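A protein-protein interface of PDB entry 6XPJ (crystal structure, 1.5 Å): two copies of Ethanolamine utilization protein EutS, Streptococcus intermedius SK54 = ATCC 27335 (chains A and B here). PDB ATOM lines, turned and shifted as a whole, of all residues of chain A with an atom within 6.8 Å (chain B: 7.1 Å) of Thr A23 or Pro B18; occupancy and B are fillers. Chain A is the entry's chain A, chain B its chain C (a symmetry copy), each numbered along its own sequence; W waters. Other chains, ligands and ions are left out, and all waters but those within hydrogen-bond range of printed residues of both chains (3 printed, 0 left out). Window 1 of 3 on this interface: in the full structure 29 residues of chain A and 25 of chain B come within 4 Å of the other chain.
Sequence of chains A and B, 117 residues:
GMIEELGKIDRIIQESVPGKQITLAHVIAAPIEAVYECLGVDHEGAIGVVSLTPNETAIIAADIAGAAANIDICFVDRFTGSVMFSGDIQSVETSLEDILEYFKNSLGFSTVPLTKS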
ATOM      1  N   GLN A  21      -4.043 -24.183  13.976  1.00  0.00           N
ATOM      2  CA  GLN A  21      -3.452 -23.042  14.694  1.00  0.00           C
ATOM      3  C   GLN A  21      -2.548 -23.509  15.816  1.00  0.00           C
ATOM      4  O   GLN A  21      -2.892 -24.432  16.562  1.00  0.00           O
ATOM      5  CB  GLN A  21      -4.558 -22.130  15.245  1.00  0.00           C
ATOM      6  CG  GLN A  21      -4.058 -20.900  15.998  1.00  0.00           C
ATOM      7  CD  GLN A  21      -5.194 -19.977  16.350  1.00  0.00           C
ATOM      8  OE1 GLN A  21      -5.587 -19.825  17.527  1.00  0.00           O
ATOM      9  NE2 GLN A  21      -5.728 -19.370  15.310  1.00  0.00           N
ATOM     10  N   ILE A  22      -1.436 -22.810  15.968  1.00  0.00           N
ATOM     11  CA  ILE A  22      -0.665 -22.808  17.234  1.00  0.00           C
ATOM     12  C   ILE A  22      -1.052 -21.521  17.955  1.00  0.00           C
ATOM     13  O   ILE A  22      -0.868 -20.418  17.402  1.00  0.00           O
ATOM     14  CB  ILE A  22       0.859 -22.886  17.014  1.00  0.00           C
ATOM     15  CG1 ILE A  22       1.258 -24.223  16.385  1.00  0.00           C
ATOM     16  CG2 ILE A  22       1.586 -22.667  18.326  1.00  0.00           C
ATOM     17  CD1 ILE A  22       2.767 -24.409  16.219  1.00  0.00           C
ATOM     18  N   THR A  23      -1.601 -21.665  19.151  1.00  0.00           N
ATOM     19  CA  THR A  23      -2.113 -20.523  19.937  1.00  0.00           C
ATOM     20  C   THR A  23      -1.122 -20.138  21.039  1.00  0.00           C
ATOM     21  O   THR A  23      -1.248 -19.046  21.598  1.00  0.00           O
ATOM     22  CB  THR A  23      -3.492 -20.819  20.530  1.00  0.00           C
ATOM     23  OG1 THR A  23      -4.324 -21.406  19.526  1.00  0.00           O
ATOM     24  CG2 THR A  23      -4.183 -19.591  21.065  1.00  0.00           C
ATOM     25  N   LEU A  24      -0.133 -20.971  21.336  1.00  0.00           N
ATOM     26  CA  LEU A  24       0.880 -20.675  22.358  1.00  0.00           C
ATOM     27  C   LEU A  24       2.143 -21.409  21.982  1.00  0.00           C
ATOM     28  O   LEU A  24       2.083 -22.605  21.668  1.00  0.00           O
ATOM     29  CB  LEU A  24       0.361 -21.104  23.724  1.00  0.00           C
ATOM     30  CG  LEU A  24       1.256 -20.742  24.897  1.00  0.00           C
ATOM     31  CD1 LEU A  24       1.225 -19.243  25.153  1.00  0.00           C
ATOM     32  CD2 LEU A  24       0.794 -21.524  26.126  1.00  0.00           C
ATOM     33  N   ALA A  25       3.255 -20.688  22.048  1.00  0.00           N
ATOM     34  CA  ALA A  25       4.606 -21.238  21.846  1.00  0.00           C
ATOM     35  C   ALA A  25       5.506 -20.437  22.764  1.00  0.00           C
ATOM     36  O   ALA A  25       5.967 -19.346  22.380  1.00  0.00           O
ATOM     37  CB  ALA A  25       5.011 -21.131  20.388  1.00  0.00           C
ATOM     38  N   VAL A  50       3.433 -25.507  24.460  1.00  0.00           N
ATOM     39  CA  VAL A  50       2.786 -25.354  23.136  1.00  0.00           C
ATOM     40  C   VAL A  50       1.320 -25.754  23.239  1.00  0.00           C
ATOM     41  O   VAL A  50       0.994 -26.810  23.827  1.00  0.00           O
ATOM     42  CB  VAL A  50       3.512 -26.184  22.068  1.00  0.00           C
ATOM     43  CG1 VAL A  50       2.997 -25.885  20.679  1.00  0.00           C
ATOM     44  CG2 VAL A  50       5.004 -25.962  22.163  1.00  0.00           C
ATOM     45  N   SER A  51       0.474 -24.929  22.646  1.00  0.00           N
ATOM     46  CA  SER A  51      -0.986 -25.150  22.475  1.00  0.00           C
ATOM     47  C   SER A  51      -1.245 -25.263  20.985  1.00  0.00           C
ATOM     48  O   SER A  51      -0.921 -24.290  20.266  1.00  0.00           O
ATOM     49  CB  SER A  51      -1.797 -23.995  23.028  1.00  0.00           C
ATOM     50  OG  SER A  51      -3.192 -24.249  22.846  1.00  0.00           O
ATOM     51  N   LEU A  52      -1.842 -26.370  20.562  1.00  0.00           N
ATOM     52  CA  LEU A  52      -2.077 -26.675  19.133  1.00  0.00           C
ATOM     53  C   LEU A  52      -3.530 -27.089  18.903  1.00  0.00           C
ATOM     54  O   LEU A  52      -4.167 -27.698  19.773  1.00  0.00           O
ATOM     55  CB  LEU A  52      -1.158 -27.817  18.684  1.00  0.00           C
ATOM     56  CG  LEU A  52       0.325 -27.671  19.008  1.00  0.00           C
ATOM     57  CD1 LEU A  52       0.709 -28.453  20.260  1.00  0.00           C
ATOM     58  CD2 LEU A  52       1.156 -28.087  17.820  1.00  0.00           C
ATOM     59  N   THR A  53      -3.971 -26.871  17.678  1.00  0.00           N
ATOM     60  CA  THR A  53      -5.273 -27.306  17.154  1.00  0.00           C
ATOM     61  C   THR A  53      -5.070 -27.650  15.693  1.00  0.00           C
ATOM     62  O   THR A  53      -4.464 -26.860  14.981  1.00  0.00           O
ATOM     63  CB  THR A  53      -6.295 -26.162  17.255  1.00  0.00           C
ATOM     64  OG1 THR A  53      -6.220 -25.598  18.580  1.00  0.00           O
ATOM     65  CG2 THR A  53      -7.656 -26.672  16.837  1.00  0.00           C
ATOM     66  N   SER A 110      -2.084 -21.171  11.137  1.00  0.00           N
ATOM     67  CA  SER A 110      -1.997 -19.881  11.853  1.00  0.00           C
ATOM     68  C   SER A 110      -1.056 -20.069  13.041  1.00  0.00           C
ATOM     69  O   SER A 110      -1.098 -21.110  13.669  1.00  0.00           O
ATOM     70  CB  SER A 110      -3.342 -19.396  12.280  1.00  0.00           C
ATOM     71  OG  SER A 110      -4.131 -19.101  11.146  1.00  0.00           O
ATOM     72  N   THR A 111      -0.194 -19.106  13.289  1.00  0.00           N
ATOM     73  CA  THR A 111       0.746 -19.216  14.413  1.00  0.00           C
ATOM     74  C   THR A 111       0.668 -17.932  15.231  1.00  0.00           C
ATOM     75  O   THR A 111      -0.160 -17.054  14.965  1.00  0.00           O
ATOM     76  CB  THR A 111       2.150 -19.610  13.936  1.00  0.00           C
ATOM     77  OG1 THR A 111       2.650 -18.616  13.041  1.00  0.00           O
ATOM     78  CG2 THR A 111       2.208 -20.948  13.241  1.00  0.00           C
ATOM     79  N   VAL A 112       1.350 -17.960  16.336  1.00  0.00           N
ATOM     80  CA  VAL A 112       1.544 -16.822  17.271  1.00  0.00           C
ATOM     81  C   VAL A 112       3.041 -16.605  17.375  1.00  0.00           C
ATOM     82  O   VAL A 112       3.877 -17.465  17.040  1.00  0.00           O
ATOM     83  CB  VAL A 112       0.935 -17.139  18.647  1.00  0.00           C
ATOM     84  CG1 VAL A 112      -0.580 -17.194  18.601  1.00  0.00           C
ATOM     85  CG2 VAL A 112       1.473 -18.442  19.209  1.00  0.00           C
ATOM     86  N   PRO A 113       3.442 -15.470  17.945  1.00  0.00           N
ATOM     87  CA  PRO A 113       4.839 -15.250  18.276  1.00  0.00           C
ATOM     88  C   PRO A 113       5.320 -16.230  19.339  1.00  0.00           C
ATOM     89  O   PRO A 113       4.541 -16.768  20.120  1.00  0.00           O
ATOM     90  CB  PRO A 113       4.907 -13.853  18.912  1.00  0.00           C
ATOM     91  CG  PRO A 113       3.530 -13.280  18.766  1.00  0.00           C
ATOM     92  CD  PRO A 113       2.572 -14.358  18.347  1.00  0.00           C
ATOM     93  N   SER B  16     -13.034 -23.920  14.700  1.00  0.00           N
ATOM     94  CA  SER B  16     -12.869 -23.550  16.115  1.00  0.00           C
ATOM     95  C   SER B  16     -11.390 -23.536  16.498  1.00  0.00           C
ATOM     96  O   SER B  16     -10.709 -24.564  16.366  1.00  0.00           O
ATOM     97  CB  SER B  16     -13.648 -24.494  16.957  1.00  0.00           C
ATOM     98  OG  SER B  16     -13.595 -24.089  18.304  1.00  0.00           O
ATOM     99  N   VAL B  17     -10.932 -22.434  17.061  1.00  0.00           N
ATOM    100  CA  VAL B  17      -9.584 -22.315  17.667  1.00  0.00           C
ATOM    101  C   VAL B  17      -9.777 -21.609  18.989  1.00  0.00           C
ATOM    102  O   VAL B  17     -10.728 -20.852  19.183  1.00  0.00           O
ATOM    103  CB  VAL B  17      -8.581 -21.561  16.775  1.00  0.00           C
ATOM    104  CG1 VAL B  17      -8.446 -22.262  15.421  1.00  0.00           C
ATOM    105  CG2 VAL B  17      -8.962 -20.105  16.600  1.00  0.00           C
ATOM    106  N   PRO B  18      -8.867 -21.785  19.957  1.00  0.00           N
ATOM    107  CA  PRO B  18      -8.973 -21.026  21.187  1.00  0.00           C
ATOM    108  C   PRO B  18      -8.583 -19.563  20.969  1.00  0.00           C
ATOM    109  O   PRO B  18      -7.729 -19.232  20.144  1.00  0.00           O
ATOM    110  CB  PRO B  18      -7.985 -21.715  22.151  1.00  0.00           C
ATOM    111  CG  PRO B  18      -7.172 -22.644  21.352  1.00  0.00           C
ATOM    112  CD  PRO B  18      -7.759 -22.739  19.959  1.00  0.00           C
ATOM    113  N   GLY B  19      -9.260 -18.690  21.694  1.00  0.00           N
ATOM    114  CA  GLY B  19      -8.863 -17.282  21.801  1.00  0.00           C
ATOM    115  C   GLY B  19      -7.750 -17.097  22.814  1.00  0.00           C
ATOM    116  O   GLY B  19      -7.200 -18.086  23.306  1.00  0.00           O
ATOM    117  N   LYS B  20      -7.437 -15.836  23.069  1.00  0.00           N
ATOM    118  CA  LYS B  20      -6.295 -15.424  23.901  1.00  0.00           C
ATOM    119  C   LYS B  20      -6.846 -14.424  24.885  1.00  0.00           C
ATOM    120  O   LYS B  20      -6.931 -13.251  24.563  1.00  0.00           O
ATOM    121  CB  LYS B  20      -5.157 -14.912  23.027  1.00  0.00           C
ATOM    122  CG  LYS B  20      -4.536 -15.991  22.170  1.00  0.00           C
ATOM    123  CD  LYS B  20      -3.602 -15.433  21.101  1.00  0.00           C
ATOM    124  CE  LYS B  20      -4.389 -14.672  20.045  1.00  0.00           C
ATOM    125  NZ  LYS B  20      -3.718 -14.635  18.720  1.00  0.00           N
ATOM    126  N   GLN B  21      -7.222 -14.893  26.073  1.00  0.00           N
ATOM    127  CA  GLN B  21      -8.020 -14.041  26.984  1.00  0.00           C
ATOM    128  C   GLN B  21      -7.844 -14.514  28.421  1.00  0.00           C
ATOM    129  O   GLN B  21      -7.840 -15.729  28.663  1.00  0.00           O
ATOM    130  CB  GLN B  21      -9.492 -14.150  26.564  1.00  0.00           C
ATOM    131  CG  GLN B  21     -10.465 -13.401  27.438  1.00  0.00           C
ATOM    132  CD  GLN B  21     -11.790 -13.251  26.728  1.00  0.00           C
ATOM    133  OE1 GLN B  21     -11.876 -12.670  25.650  1.00  0.00           O
ATOM    134  NE2 GLN B  21     -12.829 -13.750  27.364  1.00  0.00           N
ATOM    135  N   THR B  53      -7.508 -18.583  28.658  1.00  0.00           N
ATOM    136  CA  THR B  53      -7.660 -19.257  27.356  1.00  0.00           C
ATOM    137  C   THR B  53      -6.485 -18.777  26.519  1.00  0.00           C
ATOM    138  O   THR B  53      -6.216 -17.569  26.510  1.00  0.00           O
ATOM    139  CB  THR B  53      -8.997 -18.872  26.699  1.00  0.00           C
ATOM    140  OG1 THR B  53     -10.054 -19.055  27.665  1.00  0.00           O
ATOM    141  CG2 THR B  53      -9.192 -19.637  25.412  1.00  0.00           C
ATOM    142  N   PRO B  54      -5.728 -19.651  25.830  1.00  0.00           N
ATOM    143  CA  PRO B  54      -5.901 -21.102  25.871  1.00  0.00           C
ATOM    144  C   PRO B  54      -5.448 -21.700  27.212  1.00  0.00           C
ATOM    145  O   PRO B  54      -4.748 -21.057  27.994  1.00  0.00           O
ATOM    146  CB  PRO B  54      -5.005 -21.596  24.732  1.00  0.00           C
ATOM    147  CG  PRO B  54      -3.909 -20.560  24.673  1.00  0.00           C
ATOM    148  CD  PRO B  54      -4.586 -19.250  24.995  1.00  0.00           C
ATOM    149  N   ASN B  55      -5.922 -22.897  27.481  1.00  0.00           N
ATOM    150  CA  ASN B  55      -5.827 -23.466  28.843  1.00  0.00           C
ATOM    151  C   ASN B  55      -4.381 -23.713  29.270  1.00  0.00           C
ATOM    152  O   ASN B  55      -4.118 -23.687  30.467  1.00  0.00           O
ATOM    153  CB  ASN B  55      -6.621 -24.747  28.927  1.00  0.00           C
ATOM    154  CG  ASN B  55      -8.118 -24.499  28.865  1.00  0.00           C
ATOM    155  OD1 ASN B  55      -8.568 -23.367  28.989  1.00  0.00           O
ATOM    156  ND2 ASN B  55      -8.884 -25.580  28.770  1.00  0.00           N
ATOM    157  N   GLU B  56      -3.474 -23.927  28.325  1.00  0.00           N
ATOM    158  CA  GLU B  56      -2.051 -24.183  28.627  1.00  0.00           C
ATOM    159  C   GLU B  56      -1.416 -22.958  29.282  1.00  0.00           C
ATOM    160  O   GLU B  56      -0.341 -23.120  29.908  1.00  0.00           O
ATOM    161  CB  GLU B  56      -1.273 -24.552  27.355  1.00  0.00           C
ATOM    162  CG  GLU B  56      -1.707 -25.838  26.691  1.00  0.00           C
ATOM    163  CD  GLU B  56      -2.870 -25.734  25.712  1.00  0.00           C
ATOM    164  OE1 GLU B  56      -3.566 -24.635  25.632  1.00  0.00           O
ATOM    165  OE2 GLU B  56      -3.114 -26.733  25.019  1.00  0.00           O
ATOM    166  N   THR B  57      -1.997 -21.762  29.164  1.00  0.00           N
ATOM    167  CA  THR B  57      -1.397 -20.556  29.781  1.00  0.00           C
ATOM    168  C   THR B  57      -1.579 -20.592  31.305  1.00  0.00           C
ATOM    169  O   THR B  57      -0.955 -19.753  31.963  1.00  0.00           O
ATOM    170  CB  THR B  57      -1.970 -19.249  29.245  1.00  0.00           C
ATOM    171  OG1 THR B  57      -3.378 -19.147  29.519  1.00  0.00           O
ATOM    172  CG2 THR B  57      -1.704 -19.074  27.771  1.00  0.00           C
ATOM    173  N   PHE B 109      -2.968 -10.146  25.184  1.00  0.00           N
ATOM    174  CA  PHE B 109      -4.242 -10.854  25.389  1.00  0.00           C
ATOM    175  C   PHE B 109      -5.336  -9.883  25.828  1.00  0.00           C
ATOM    176  O   PHE B 109      -5.024  -8.844  26.433  1.00  0.00           O
ATOM    177  CB  PHE B 109      -4.053 -11.922  26.457  1.00  0.00           C
ATOM    178  CG  PHE B 109      -3.439 -13.213  25.983  1.00  0.00           C
ATOM    179  CD1 PHE B 109      -2.468 -13.260  24.982  1.00  0.00           C
ATOM    180  CD2 PHE B 109      -3.844 -14.398  26.584  1.00  0.00           C
ATOM    181  CE1 PHE B 109      -1.926 -14.476  24.578  1.00  0.00           C
ATOM    182  CE2 PHE B 109      -3.250 -15.594  26.218  1.00  0.00           C
ATOM    183  CZ  PHE B 109      -2.315 -15.630  25.212  1.00  0.00           C
HETATM  184  O   HOH W   1      -4.797 -27.118  22.466  1.00  0.00           O
HETATM  185  O   HOH W   2      -3.877 -17.025  17.847  1.00  0.00           O
HETATM  186  O   HOH W   3      -6.516 -17.268  18.697  1.00  0.00           O
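2 positions are printed for both chains.
Of the 11 pairs that touch across the chains among the printed residues, none has its exchanged pair printed and touching as well.
Water W2 lies within hydrogen-bond range of NZ of Lys B20 (2.5 Å) and OE1 of Gln A21 (3.3 Å).
Water W3 bridges O of Pro B18 (2.7 Å) and OE1 of Gln A21 (3.0 Å).
Water W1 lies within hydrogen-bond range of the backbone carbonyl oxygen of Leu A52 (2.8 Å), the side-chain carboxylate of Glu B56 (3.1 Å) and the side-chain hydroxyl of Ser A51 (3.3 Å).
O of Ser A51 lies within hydrogen-bond range of N of Thr A23 (2.9 Å).
The backbone carbonyl oxygen (O) of Thr A53 sits at hydrogen-bond distance from the backbone NH (N) of Gln A21.
The backbone carbonyl oxygen of Pro B54 lies within hydrogen-bond range of the side-chain hydroxyl of Thr B57, at 2.8 Å.
The backbone NH of Ser A51 is in hydrogen-bond range of the backbone carbonyl oxygen of Leu A24 (3.0 Å).
The side-chain amide oxygen (OE1) of Gln A21 is in hydrogen-bond range of the side-chain hydroxyl (OG1) of Thr A23, 2.8 Å away.
Gln A21 touches Val B17 (OE1 to CG2, 3.5 Å).
OG1 of Thr A23 touches CG of Pro B18, 3.6 Å away.
Lys B20 touches Thr A23.
Pro B54 touches Thr A23.
Leu A24 touches Glu B56 (CD2 to CB, 3.9 Å).
Thr B57 touches Leu A24 (CG2 to CD2, 3.9 Å).
Ser A51 touches Pro B54 (OG to CB, 3.7 Å).
CG2 of Thr A53 touches O of Ser B16 (3.7 Å).
OG1 of Thr A53 touches CD of Pro B18, at 3.5 Å.
The backbone carbonyl oxygen (O) of Pro B18 lies close to the side-chain amide oxygen (OE1) of Gln A21 (3.4 Å).
The side-chain hydroxyl (OG) of Ser A51 is in hydrogen-bond range of the side-chain carboxylate (OE1) of Glu B56 (2.8 Å).
Hydrophobic or aromatic side chains of chain A that line the printed part of chain B: Leu A24.
Printed residues of chain B that touch a printed residue of chain A: Ser B16, Val B17, Pro B18, Lys B20, Pro B54, Glu B56 and Thr B57.
Hydrophobic or aromatic side chains of chain B that line the printed part of chain A: Val B17, Pro B18 and Pro B54.
Among the printed residues, 11 pairs touch across the chains.
Ile A22 touches none of the printed residues of chain B.
Of the printed residues of chain B, Thr A23 touches Pro B18, Lys B20 and Pro B54.
Printed residues of chain B within 4 Å of Ser A51: Pro B54 and Glu B56.
Pro B18 touches just these residues of chain A: Gln A21 (3.4 Å), Thr A23 (3.6 Å) and Thr A53 (3.5 Å).
Gln B21 touches none of the printed residues of chain A.
Of the printed residues of chain A, Pro B54 touches Thr A23 (3.7 Å) and Ser A51 (3.7 Å).
Of the printed residues of chain A, Thr B57 touches Leu A24.
The nearest residue of chain B that does not touch Thr A23 is Gly B19 (4.05 Å).
The nearest printed residue of chain B that does not touch Thr A53 is Val B17 (4.7 Å).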
